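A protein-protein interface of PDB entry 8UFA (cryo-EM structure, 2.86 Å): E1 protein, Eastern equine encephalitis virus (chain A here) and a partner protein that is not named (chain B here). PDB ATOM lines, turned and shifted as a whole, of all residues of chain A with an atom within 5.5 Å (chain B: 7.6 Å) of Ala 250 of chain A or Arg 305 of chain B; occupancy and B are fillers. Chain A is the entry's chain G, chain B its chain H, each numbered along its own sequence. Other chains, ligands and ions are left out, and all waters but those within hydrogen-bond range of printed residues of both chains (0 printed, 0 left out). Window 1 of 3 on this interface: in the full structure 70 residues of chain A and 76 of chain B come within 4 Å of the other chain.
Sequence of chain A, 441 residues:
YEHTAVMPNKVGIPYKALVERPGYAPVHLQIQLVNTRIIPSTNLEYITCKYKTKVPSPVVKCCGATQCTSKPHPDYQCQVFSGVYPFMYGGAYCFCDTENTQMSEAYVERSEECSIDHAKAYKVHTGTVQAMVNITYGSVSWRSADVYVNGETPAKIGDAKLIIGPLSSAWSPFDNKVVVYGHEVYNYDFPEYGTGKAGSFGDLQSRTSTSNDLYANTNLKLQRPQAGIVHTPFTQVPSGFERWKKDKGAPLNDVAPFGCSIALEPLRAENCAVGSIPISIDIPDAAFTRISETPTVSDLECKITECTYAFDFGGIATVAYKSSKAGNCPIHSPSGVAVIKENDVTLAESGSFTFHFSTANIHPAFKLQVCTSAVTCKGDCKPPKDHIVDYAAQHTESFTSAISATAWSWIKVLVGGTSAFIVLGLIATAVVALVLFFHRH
OD2 of Asp 254 of chain A lies within salt-bridge range of NH2 of Arg 135 of chain B (3.3 Å).
The guanidinium group (NH2) of Arg 135 of chain B lies within hydrogen-bond range of the side-chain hydroxyl (OG1) of Thr 293 of chain B (2.7 Å).
The backbone carbonyl oxygen (O) of Arg 135 of chain B lies within hydrogen-bond range of the backbone NH (N) of Leu 291 of chain B (3.0 Å).
Among the printed residues, merely in contact across the chains: Gly 249 of chain A with Arg 305 of chain B (3.8 Å), Ala 250 of chain A with Arg 305 of chain B (3.7 Å) and Val 255 of chain A with Pro 303 of chain B (3.7 Å).
Lys 248 of chain A touches none of the printed residues of chain B.
Ala 250 of chain A touches just one residue of chain B: Arg 305.
Of the printed residues of chain B, Asp 254 of chain A touches Arg 135.
Of the printed residues of chain A, Arg 135 of chain B touches Asp 254 (3.3 Å).
Asn 302 of chain B touches none of the printed residues of chain A.
Printed residues of chain A within 4 Å of Pro 303 of chain B: Val 255.
Arg 305 of chain B touches just these residues of chain A: Gly 249 and Ala 250.
The nearest residue of chain B that does not touch Ala 250 of chain A is Pro 303 of chain B (6.2 Å).
The nearest printed residue of chain B that does not touch Gly 249 of chain A is Leu 291 of chain B (7.0 Å).
Printed residues of chain A that touch a printed residue of chain B: Gly 249, Ala 250, Asp 254 and Val 255.
Along chain A the printed residues that touch a printed residue of chain B span positions 249 to 255.
Of the 13 printed residues of chain B, 3 touch a printed residue of chain A.
Hydrophobic or aromatic side chains of chain B within 4 Å of the printed part of chain A: Pro 303.
Among the printed residues, Asp or Glu carboxylates within 4 Å of a Lys or Arg side-chain nitrogen of the other chain: Asp 254 of chain A with Arg 135 of chain B.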
ATOM      1  N   TYR A 186      -3.861  12.691 -16.687  1.00  0.00           N
ATOM      2  CA  TYR A 186      -4.184  12.247 -18.035  1.00  0.00           C
ATOM      3  C   TYR A 186      -5.528  11.535 -18.064  1.00  0.00           C
ATOM      4  O   TYR A 186      -5.821  10.707 -17.198  1.00  0.00           O
ATOM      5  CB  TYR A 186      -3.092  11.313 -18.565  1.00  0.00           C
ATOM      6  CG  TYR A 186      -1.747  11.983 -18.692  1.00  0.00           C
ATOM      7  CD1 TYR A 186      -0.917  12.118 -17.597  1.00  0.00           C
ATOM      8  CD2 TYR A 186      -1.303  12.460 -19.911  1.00  0.00           C
ATOM      9  CE1 TYR A 186       0.309  12.715 -17.707  1.00  0.00           C
ATOM     10  CE2 TYR A 186      -0.081  13.061 -20.031  1.00  0.00           C
ATOM     11  CZ  TYR A 186       0.723  13.188 -18.926  1.00  0.00           C
ATOM     12  OH  TYR A 186       1.942  13.806 -19.034  1.00  0.00           O
ATOM     13  N   LYS A 248       3.035   9.308 -23.585  1.00  0.00           N
ATOM     14  CA  LYS A 248       1.876   9.712 -22.792  1.00  0.00           C
ATOM     15  C   LYS A 248       1.124  10.876 -23.429  1.00  0.00           C
ATOM     16  O   LYS A 248      -0.090  11.011 -23.228  1.00  0.00           O
ATOM     17  CB  LYS A 248       2.306  10.045 -21.362  1.00  0.00           C
ATOM     18  CG  LYS A 248       3.257  11.206 -21.206  1.00  0.00           C
ATOM     19  CD  LYS A 248       3.724  11.268 -19.766  1.00  0.00           C
ATOM     20  CE  LYS A 248       4.587  12.475 -19.488  1.00  0.00           C
ATOM     21  NZ  LYS A 248       5.879  12.422 -20.209  1.00  0.00           N
ATOM     22  N   GLY A 249       1.809  11.720 -24.197  1.00  0.00           N
ATOM     23  CA  GLY A 249       1.136  12.797 -24.905  1.00  0.00           C
ATOM     24  C   GLY A 249       0.858  14.030 -24.057  1.00  0.00           C
ATOM     25  O   GLY A 249       1.535  14.308 -23.066  1.00  0.00           O
ATOM     26  N   ALA A 250      -0.164  14.783 -24.474  1.00  0.00           N
ATOM     27  CA  ALA A 250      -0.537  16.027 -23.805  1.00  0.00           C
ATOM     28  C   ALA A 250      -1.346  15.743 -22.542  1.00  0.00           C
ATOM     29  O   ALA A 250      -2.346  15.022 -22.603  1.00  0.00           O
ATOM     30  CB  ALA A 250      -1.350  16.912 -24.741  1.00  0.00           C
ATOM     31  N   PRO A 251      -0.952  16.286 -21.392  1.00  0.00           N
ATOM     32  CA  PRO A 251      -1.723  16.061 -20.170  1.00  0.00           C
ATOM     33  C   PRO A 251      -2.998  16.883 -20.151  1.00  0.00           C
ATOM     34  O   PRO A 251      -3.170  17.845 -20.900  1.00  0.00           O
ATOM     35  CB  PRO A 251      -0.765  16.508 -19.064  1.00  0.00           C
ATOM     36  CG  PRO A 251       0.056  17.548 -19.704  1.00  0.00           C
ATOM     37  CD  PRO A 251       0.238  17.113 -21.128  1.00  0.00           C
ATOM     38  N   LEU A 252      -3.910  16.479 -19.268  1.00  0.00           N
ATOM     39  CA  LEU A 252      -5.134  17.245 -19.075  1.00  0.00           C
ATOM     40  C   LEU A 252      -4.817  18.667 -18.633  1.00  0.00           C
ATOM     41  O   LEU A 252      -5.570  19.600 -18.934  1.00  0.00           O
ATOM     42  CB  LEU A 252      -6.024  16.535 -18.055  1.00  0.00           C
ATOM     43  CG  LEU A 252      -7.429  17.082 -17.822  1.00  0.00           C
ATOM     44  CD1 LEU A 252      -8.204  17.143 -19.119  1.00  0.00           C
ATOM     45  CD2 LEU A 252      -8.142  16.212 -16.810  1.00  0.00           C
ATOM     46  N   ASP A 254      -2.766  20.610 -19.866  1.00  0.00           N
ATOM     47  CA  ASP A 254      -2.520  21.434 -21.042  1.00  0.00           C
ATOM     48  C   ASP A 254      -3.682  21.513 -22.024  1.00  0.00           C
ATOM     49  O   ASP A 254      -3.678  22.406 -22.878  1.00  0.00           O
ATOM     50  CB  ASP A 254      -1.296  20.902 -21.801  1.00  0.00           C
ATOM     51  CG  ASP A 254      -0.012  21.035 -21.009  1.00  0.00           C
ATOM     52  OD1 ASP A 254       0.023  21.834 -20.052  1.00  0.00           O
ATOM     53  OD2 ASP A 254       0.968  20.340 -21.349  1.00  0.00           O
ATOM     54  N   VAL A 255      -4.659  20.610 -21.950  1.00  0.00           N
ATOM     55  CA  VAL A 255      -5.739  20.550 -22.929  1.00  0.00           C
ATOM     56  C   VAL A 255      -7.120  20.761 -22.324  1.00  0.00           C
ATOM     57  O   VAL A 255      -8.106  20.761 -23.068  1.00  0.00           O
ATOM     58  CB  VAL A 255      -5.698  19.217 -23.706  1.00  0.00           C
ATOM     59  CG1 VAL A 255      -4.335  19.023 -24.336  1.00  0.00           C
ATOM     60  CG2 VAL A 255      -6.021  18.050 -22.790  1.00  0.00           C
ATOM     61  N   ARG B 135      10.274  20.762 -20.284  1.00  0.00           N
ATOM     62  CA  ARG B 135       9.737  20.824 -21.637  1.00  0.00           C
ATOM     63  C   ARG B 135      10.798  21.233 -22.655  1.00  0.00           C
ATOM     64  O   ARG B 135      10.461  21.710 -23.742  1.00  0.00           O
ATOM     65  CB  ARG B 135       8.543  21.780 -21.658  1.00  0.00           C
ATOM     66  CG  ARG B 135       7.515  21.425 -20.584  1.00  0.00           C
ATOM     67  CD  ARG B 135       6.395  22.440 -20.403  1.00  0.00           C
ATOM     68  NE  ARG B 135       5.143  22.053 -21.044  1.00  0.00           N
ATOM     69  CZ  ARG B 135       4.613  22.623 -22.118  1.00  0.00           C
ATOM     70  NH1 ARG B 135       5.284  23.502 -22.843  1.00  0.00           N
ATOM     71  NH2 ARG B 135       3.389  22.270 -22.497  1.00  0.00           N
ATOM     72  N   LEU B 291       9.336  22.503 -26.405  1.00  0.00           N
ATOM     73  CA  LEU B 291       7.929  22.176 -26.584  1.00  0.00           C
ATOM     74  C   LEU B 291       7.057  23.419 -26.446  1.00  0.00           C
ATOM     75  O   LEU B 291       7.108  24.111 -25.424  1.00  0.00           O
ATOM     76  CB  LEU B 291       7.520  21.116 -25.564  1.00  0.00           C
ATOM     77  CG  LEU B 291       6.057  20.684 -25.532  1.00  0.00           C
ATOM     78  CD1 LEU B 291       5.654  20.044 -26.836  1.00  0.00           C
ATOM     79  CD2 LEU B 291       5.838  19.731 -24.382  1.00  0.00           C
ATOM     80  N   LEU B 292       6.255  23.694 -27.471  1.00  0.00           N
ATOM     81  CA  LEU B 292       5.269  24.766 -27.463  1.00  0.00           C
ATOM     82  C   LEU B 292       3.873  24.159 -27.467  1.00  0.00           C
ATOM     83  O   LEU B 292       3.560  23.328 -28.323  1.00  0.00           O
ATOM     84  CB  LEU B 292       5.444  25.683 -28.674  1.00  0.00           C
ATOM     85  CG  LEU B 292       4.419  26.811 -28.834  1.00  0.00           C
ATOM     86  CD1 LEU B 292       4.656  27.917 -27.827  1.00  0.00           C
ATOM     87  CD2 LEU B 292       4.441  27.344 -30.250  1.00  0.00           C
ATOM     88  N   THR B 293       3.036  24.574 -26.517  1.00  0.00           N
ATOM     89  CA  THR B 293       1.655  24.122 -26.453  1.00  0.00           C
ATOM     90  C   THR B 293       0.725  25.310 -26.265  1.00  0.00           C
ATOM     91  O   THR B 293       1.076  26.295 -25.613  1.00  0.00           O
ATOM     92  CB  THR B 293       1.445  23.122 -25.313  1.00  0.00           C
ATOM     93  OG1 THR B 293       1.793  23.731 -24.066  1.00  0.00           O
ATOM     94  CG2 THR B 293       2.300  21.895 -25.527  1.00  0.00           C
ATOM     95  N   THR B 294      -0.468  25.206 -26.848  1.00  0.00           N
ATOM     96  CA  THR B 294      -1.484  26.242 -26.728  1.00  0.00           C
ATOM     97  C   THR B 294      -2.855  25.597 -26.580  1.00  0.00           C
ATOM     98  O   THR B 294      -3.066  24.443 -26.954  1.00  0.00           O
ATOM     99  CB  THR B 294      -1.492  27.191 -27.939  1.00  0.00           C
ATOM    100  OG1 THR B 294      -2.090  26.532 -29.063  1.00  0.00           O
ATOM    101  CG2 THR B 294      -0.084  27.613 -28.304  1.00  0.00           C
ATOM    102  N   ASN B 302      -9.272  23.246 -28.546  1.00  0.00           N
ATOM    103  CA  ASN B 302      -8.511  23.215 -29.794  1.00  0.00           C
ATOM    104  C   ASN B 302      -7.010  23.218 -29.481  1.00  0.00           C
ATOM    105  O   ASN B 302      -6.277  24.105 -29.944  1.00  0.00           O
ATOM    106  CB  ASN B 302      -8.890  24.381 -30.700  1.00  0.00           C
ATOM    107  CG  ASN B 302      -8.282  24.270 -32.081  1.00  0.00           C
ATOM    108  OD1 ASN B 302      -7.886  23.188 -32.513  1.00  0.00           O
ATOM    109  ND2 ASN B 302      -8.203  25.395 -32.783  1.00  0.00           N
ATOM    110  N   PRO B 303      -6.524  22.257 -28.698  1.00  0.00           N
ATOM    111  CA  PRO B 303      -5.131  22.290 -28.241  1.00  0.00           C
ATOM    112  C   PRO B 303      -4.119  22.052 -29.352  1.00  0.00           C
ATOM    113  O   PRO B 303      -4.396  21.388 -30.351  1.00  0.00           O
ATOM    114  CB  PRO B 303      -5.079  21.165 -27.203  1.00  0.00           C
ATOM    115  CG  PRO B 303      -6.114  20.212 -27.648  1.00  0.00           C
ATOM    116  CD  PRO B 303      -7.216  21.039 -28.240  1.00  0.00           C
ATOM    117  N   THR B 304      -2.927  22.618 -29.153  1.00  0.00           N
ATOM    118  CA  THR B 304      -1.800  22.479 -30.066  1.00  0.00           C
ATOM    119  C   THR B 304      -0.582  22.004 -29.283  1.00  0.00           C
ATOM    120  O   THR B 304      -0.373  22.421 -28.142  1.00  0.00           O
ATOM    121  CB  THR B 304      -1.485  23.804 -30.770  1.00  0.00           C
ATOM    122  OG1 THR B 304      -2.637  24.245 -31.497  1.00  0.00           O
ATOM    123  CG2 THR B 304      -0.319  23.642 -31.732  1.00  0.00           C
ATOM    124  N   ARG B 305       0.203  21.115 -29.890  1.00  0.00           N
ATOM    125  CA  ARG B 305       1.412  20.581 -29.262  1.00  0.00           C
ATOM    126  C   ARG B 305       2.463  20.319 -30.328  1.00  0.00           C
ATOM    127  O   ARG B 305       2.209  19.559 -31.266  1.00  0.00           O
ATOM    128  CB  ARG B 305       1.101  19.290 -28.501  1.00  0.00           C
ATOM    129  CG  ARG B 305       2.300  18.658 -27.818  1.00  0.00           C
ATOM    130  CD  ARG B 305       1.922  17.350 -27.152  1.00  0.00           C
ATOM    131  NE  ARG B 305       3.034  16.750 -26.426  1.00  0.00           N
ATOM    132  CZ  ARG B 305       3.330  16.990 -25.157  1.00  0.00           C
ATOM    133  NH1 ARG B 305       2.624  17.840 -24.428  1.00  0.00           N
ATOM    134  NH2 ARG B 305       4.368  16.368 -24.606  1.00  0.00           N
ATOM    135  N   GLN B 306       3.634  20.944 -30.199  1.00  0.00           N
ATOM    136  CA  GLN B 306       4.716  20.709 -31.143  1.00  0.00           C
ATOM    137  C   GLN B 306       6.064  21.006 -30.503  1.00  0.00           C
ATOM    138  O   GLN B 306       6.187  21.936 -29.702  1.00  0.00           O
ATOM    139  CB  GLN B 306       4.542  21.553 -32.407  1.00  0.00           C
ATOM    140  CG  GLN B 306       4.452  23.039 -32.154  1.00  0.00           C
ATOM    141  CD  GLN B 306       4.157  23.809 -33.420  1.00  0.00           C
ATOM    142  OE1 GLN B 306       4.929  23.769 -34.376  1.00  0.00           O
ATOM    143  NE2 GLN B 306       3.033  24.515 -33.433  1.00  0.00           N
ATOM    144  N   TRP B 307       7.068  20.212 -30.870  1.00  0.00           N
ATOM    145  CA  TRP B 307       8.446  20.413 -30.443  1.00  0.00           C
ATOM    146  C   TRP B 307       9.161  21.221 -31.516  1.00  0.00           C
ATOM    147  O   TRP B 307       9.153  20.843 -32.692  1.00  0.00           O
ATOM    148  CB  TRP B 307       9.164  19.080 -30.224  1.00  0.00           C
ATOM    149  CG  TRP B 307       8.778  18.378 -28.970  1.00  0.00           C
ATOM    150  CD1 TRP B 307       7.774  17.472 -28.817  1.00  0.00           C
ATOM    151  CD2 TRP B 307       9.387  18.524 -27.684  1.00  0.00           C
ATOM    152  NE1 TRP B 307       7.721  17.041 -27.519  1.00  0.00           N
ATOM    153  CE2 TRP B 307       8.701  17.672 -26.801  1.00  0.00           C
ATOM    154  CE3 TRP B 307      10.444  19.292 -27.194  1.00  0.00           C
ATOM    155  CZ2 TRP B 307       9.037  17.566 -25.455  1.00  0.00           C
ATOM    156  CZ3 TRP B 307      10.779  19.184 -25.858  1.00  0.00           C
ATOM    157  CH2 TRP B 307      10.073  18.333 -25.004  1.00  0.00           C
ATOM    158  N   ILE B 308       9.774  22.326 -31.111  1.00  0.00           N
ATOM    159  CA  ILE B 308      10.408  23.260 -32.032  1.00  0.00           C
ATOM    160  C   ILE B 308      11.917  23.187 -31.841  1.00  0.00           C
ATOM    161  O   ILE B 308      12.433  23.485 -30.757  1.00  0.00           O
ATOM    162  CB  ILE B 308       9.861  24.679 -31.827  1.00  0.00           C
ATOM    163  CG1 ILE B 308       8.364  24.660 -32.142  1.00  0.00           C
ATOM    164  CG2 ILE B 308      10.595  25.684 -32.706  1.00  0.00           C
ATOM    165  CD1 ILE B 308       7.653  25.921 -31.867  1.00  0.00           C
ATOM    166  N   PHE B 316      -1.249  31.906 -34.095  1.00  0.00           N
ATOM    167  CA  PHE B 316      -2.403  31.355 -33.401  1.00  0.00           C
ATOM    168  C   PHE B 316      -3.568  32.335 -33.434  1.00  0.00           C
ATOM    169  O   PHE B 316      -3.377  33.545 -33.285  1.00  0.00           O
ATOM    170  CB  PHE B 316      -2.050  31.013 -31.953  1.00  0.00           C
ATOM    171  CG  PHE B 316      -0.925  30.038 -31.829  1.00  0.00           C
ATOM    172  CD1 PHE B 316      -1.103  28.710 -32.162  1.00  0.00           C
ATOM    173  CD2 PHE B 316       0.310  30.448 -31.376  1.00  0.00           C
ATOM    174  CE1 PHE B 316      -0.071  27.813 -32.045  1.00  0.00           C
ATOM    175  CE2 PHE B 316       1.347  29.557 -31.263  1.00  0.00           C
ATOM    176  CZ  PHE B 316       1.159  28.235 -31.599  1.00  0.00           C
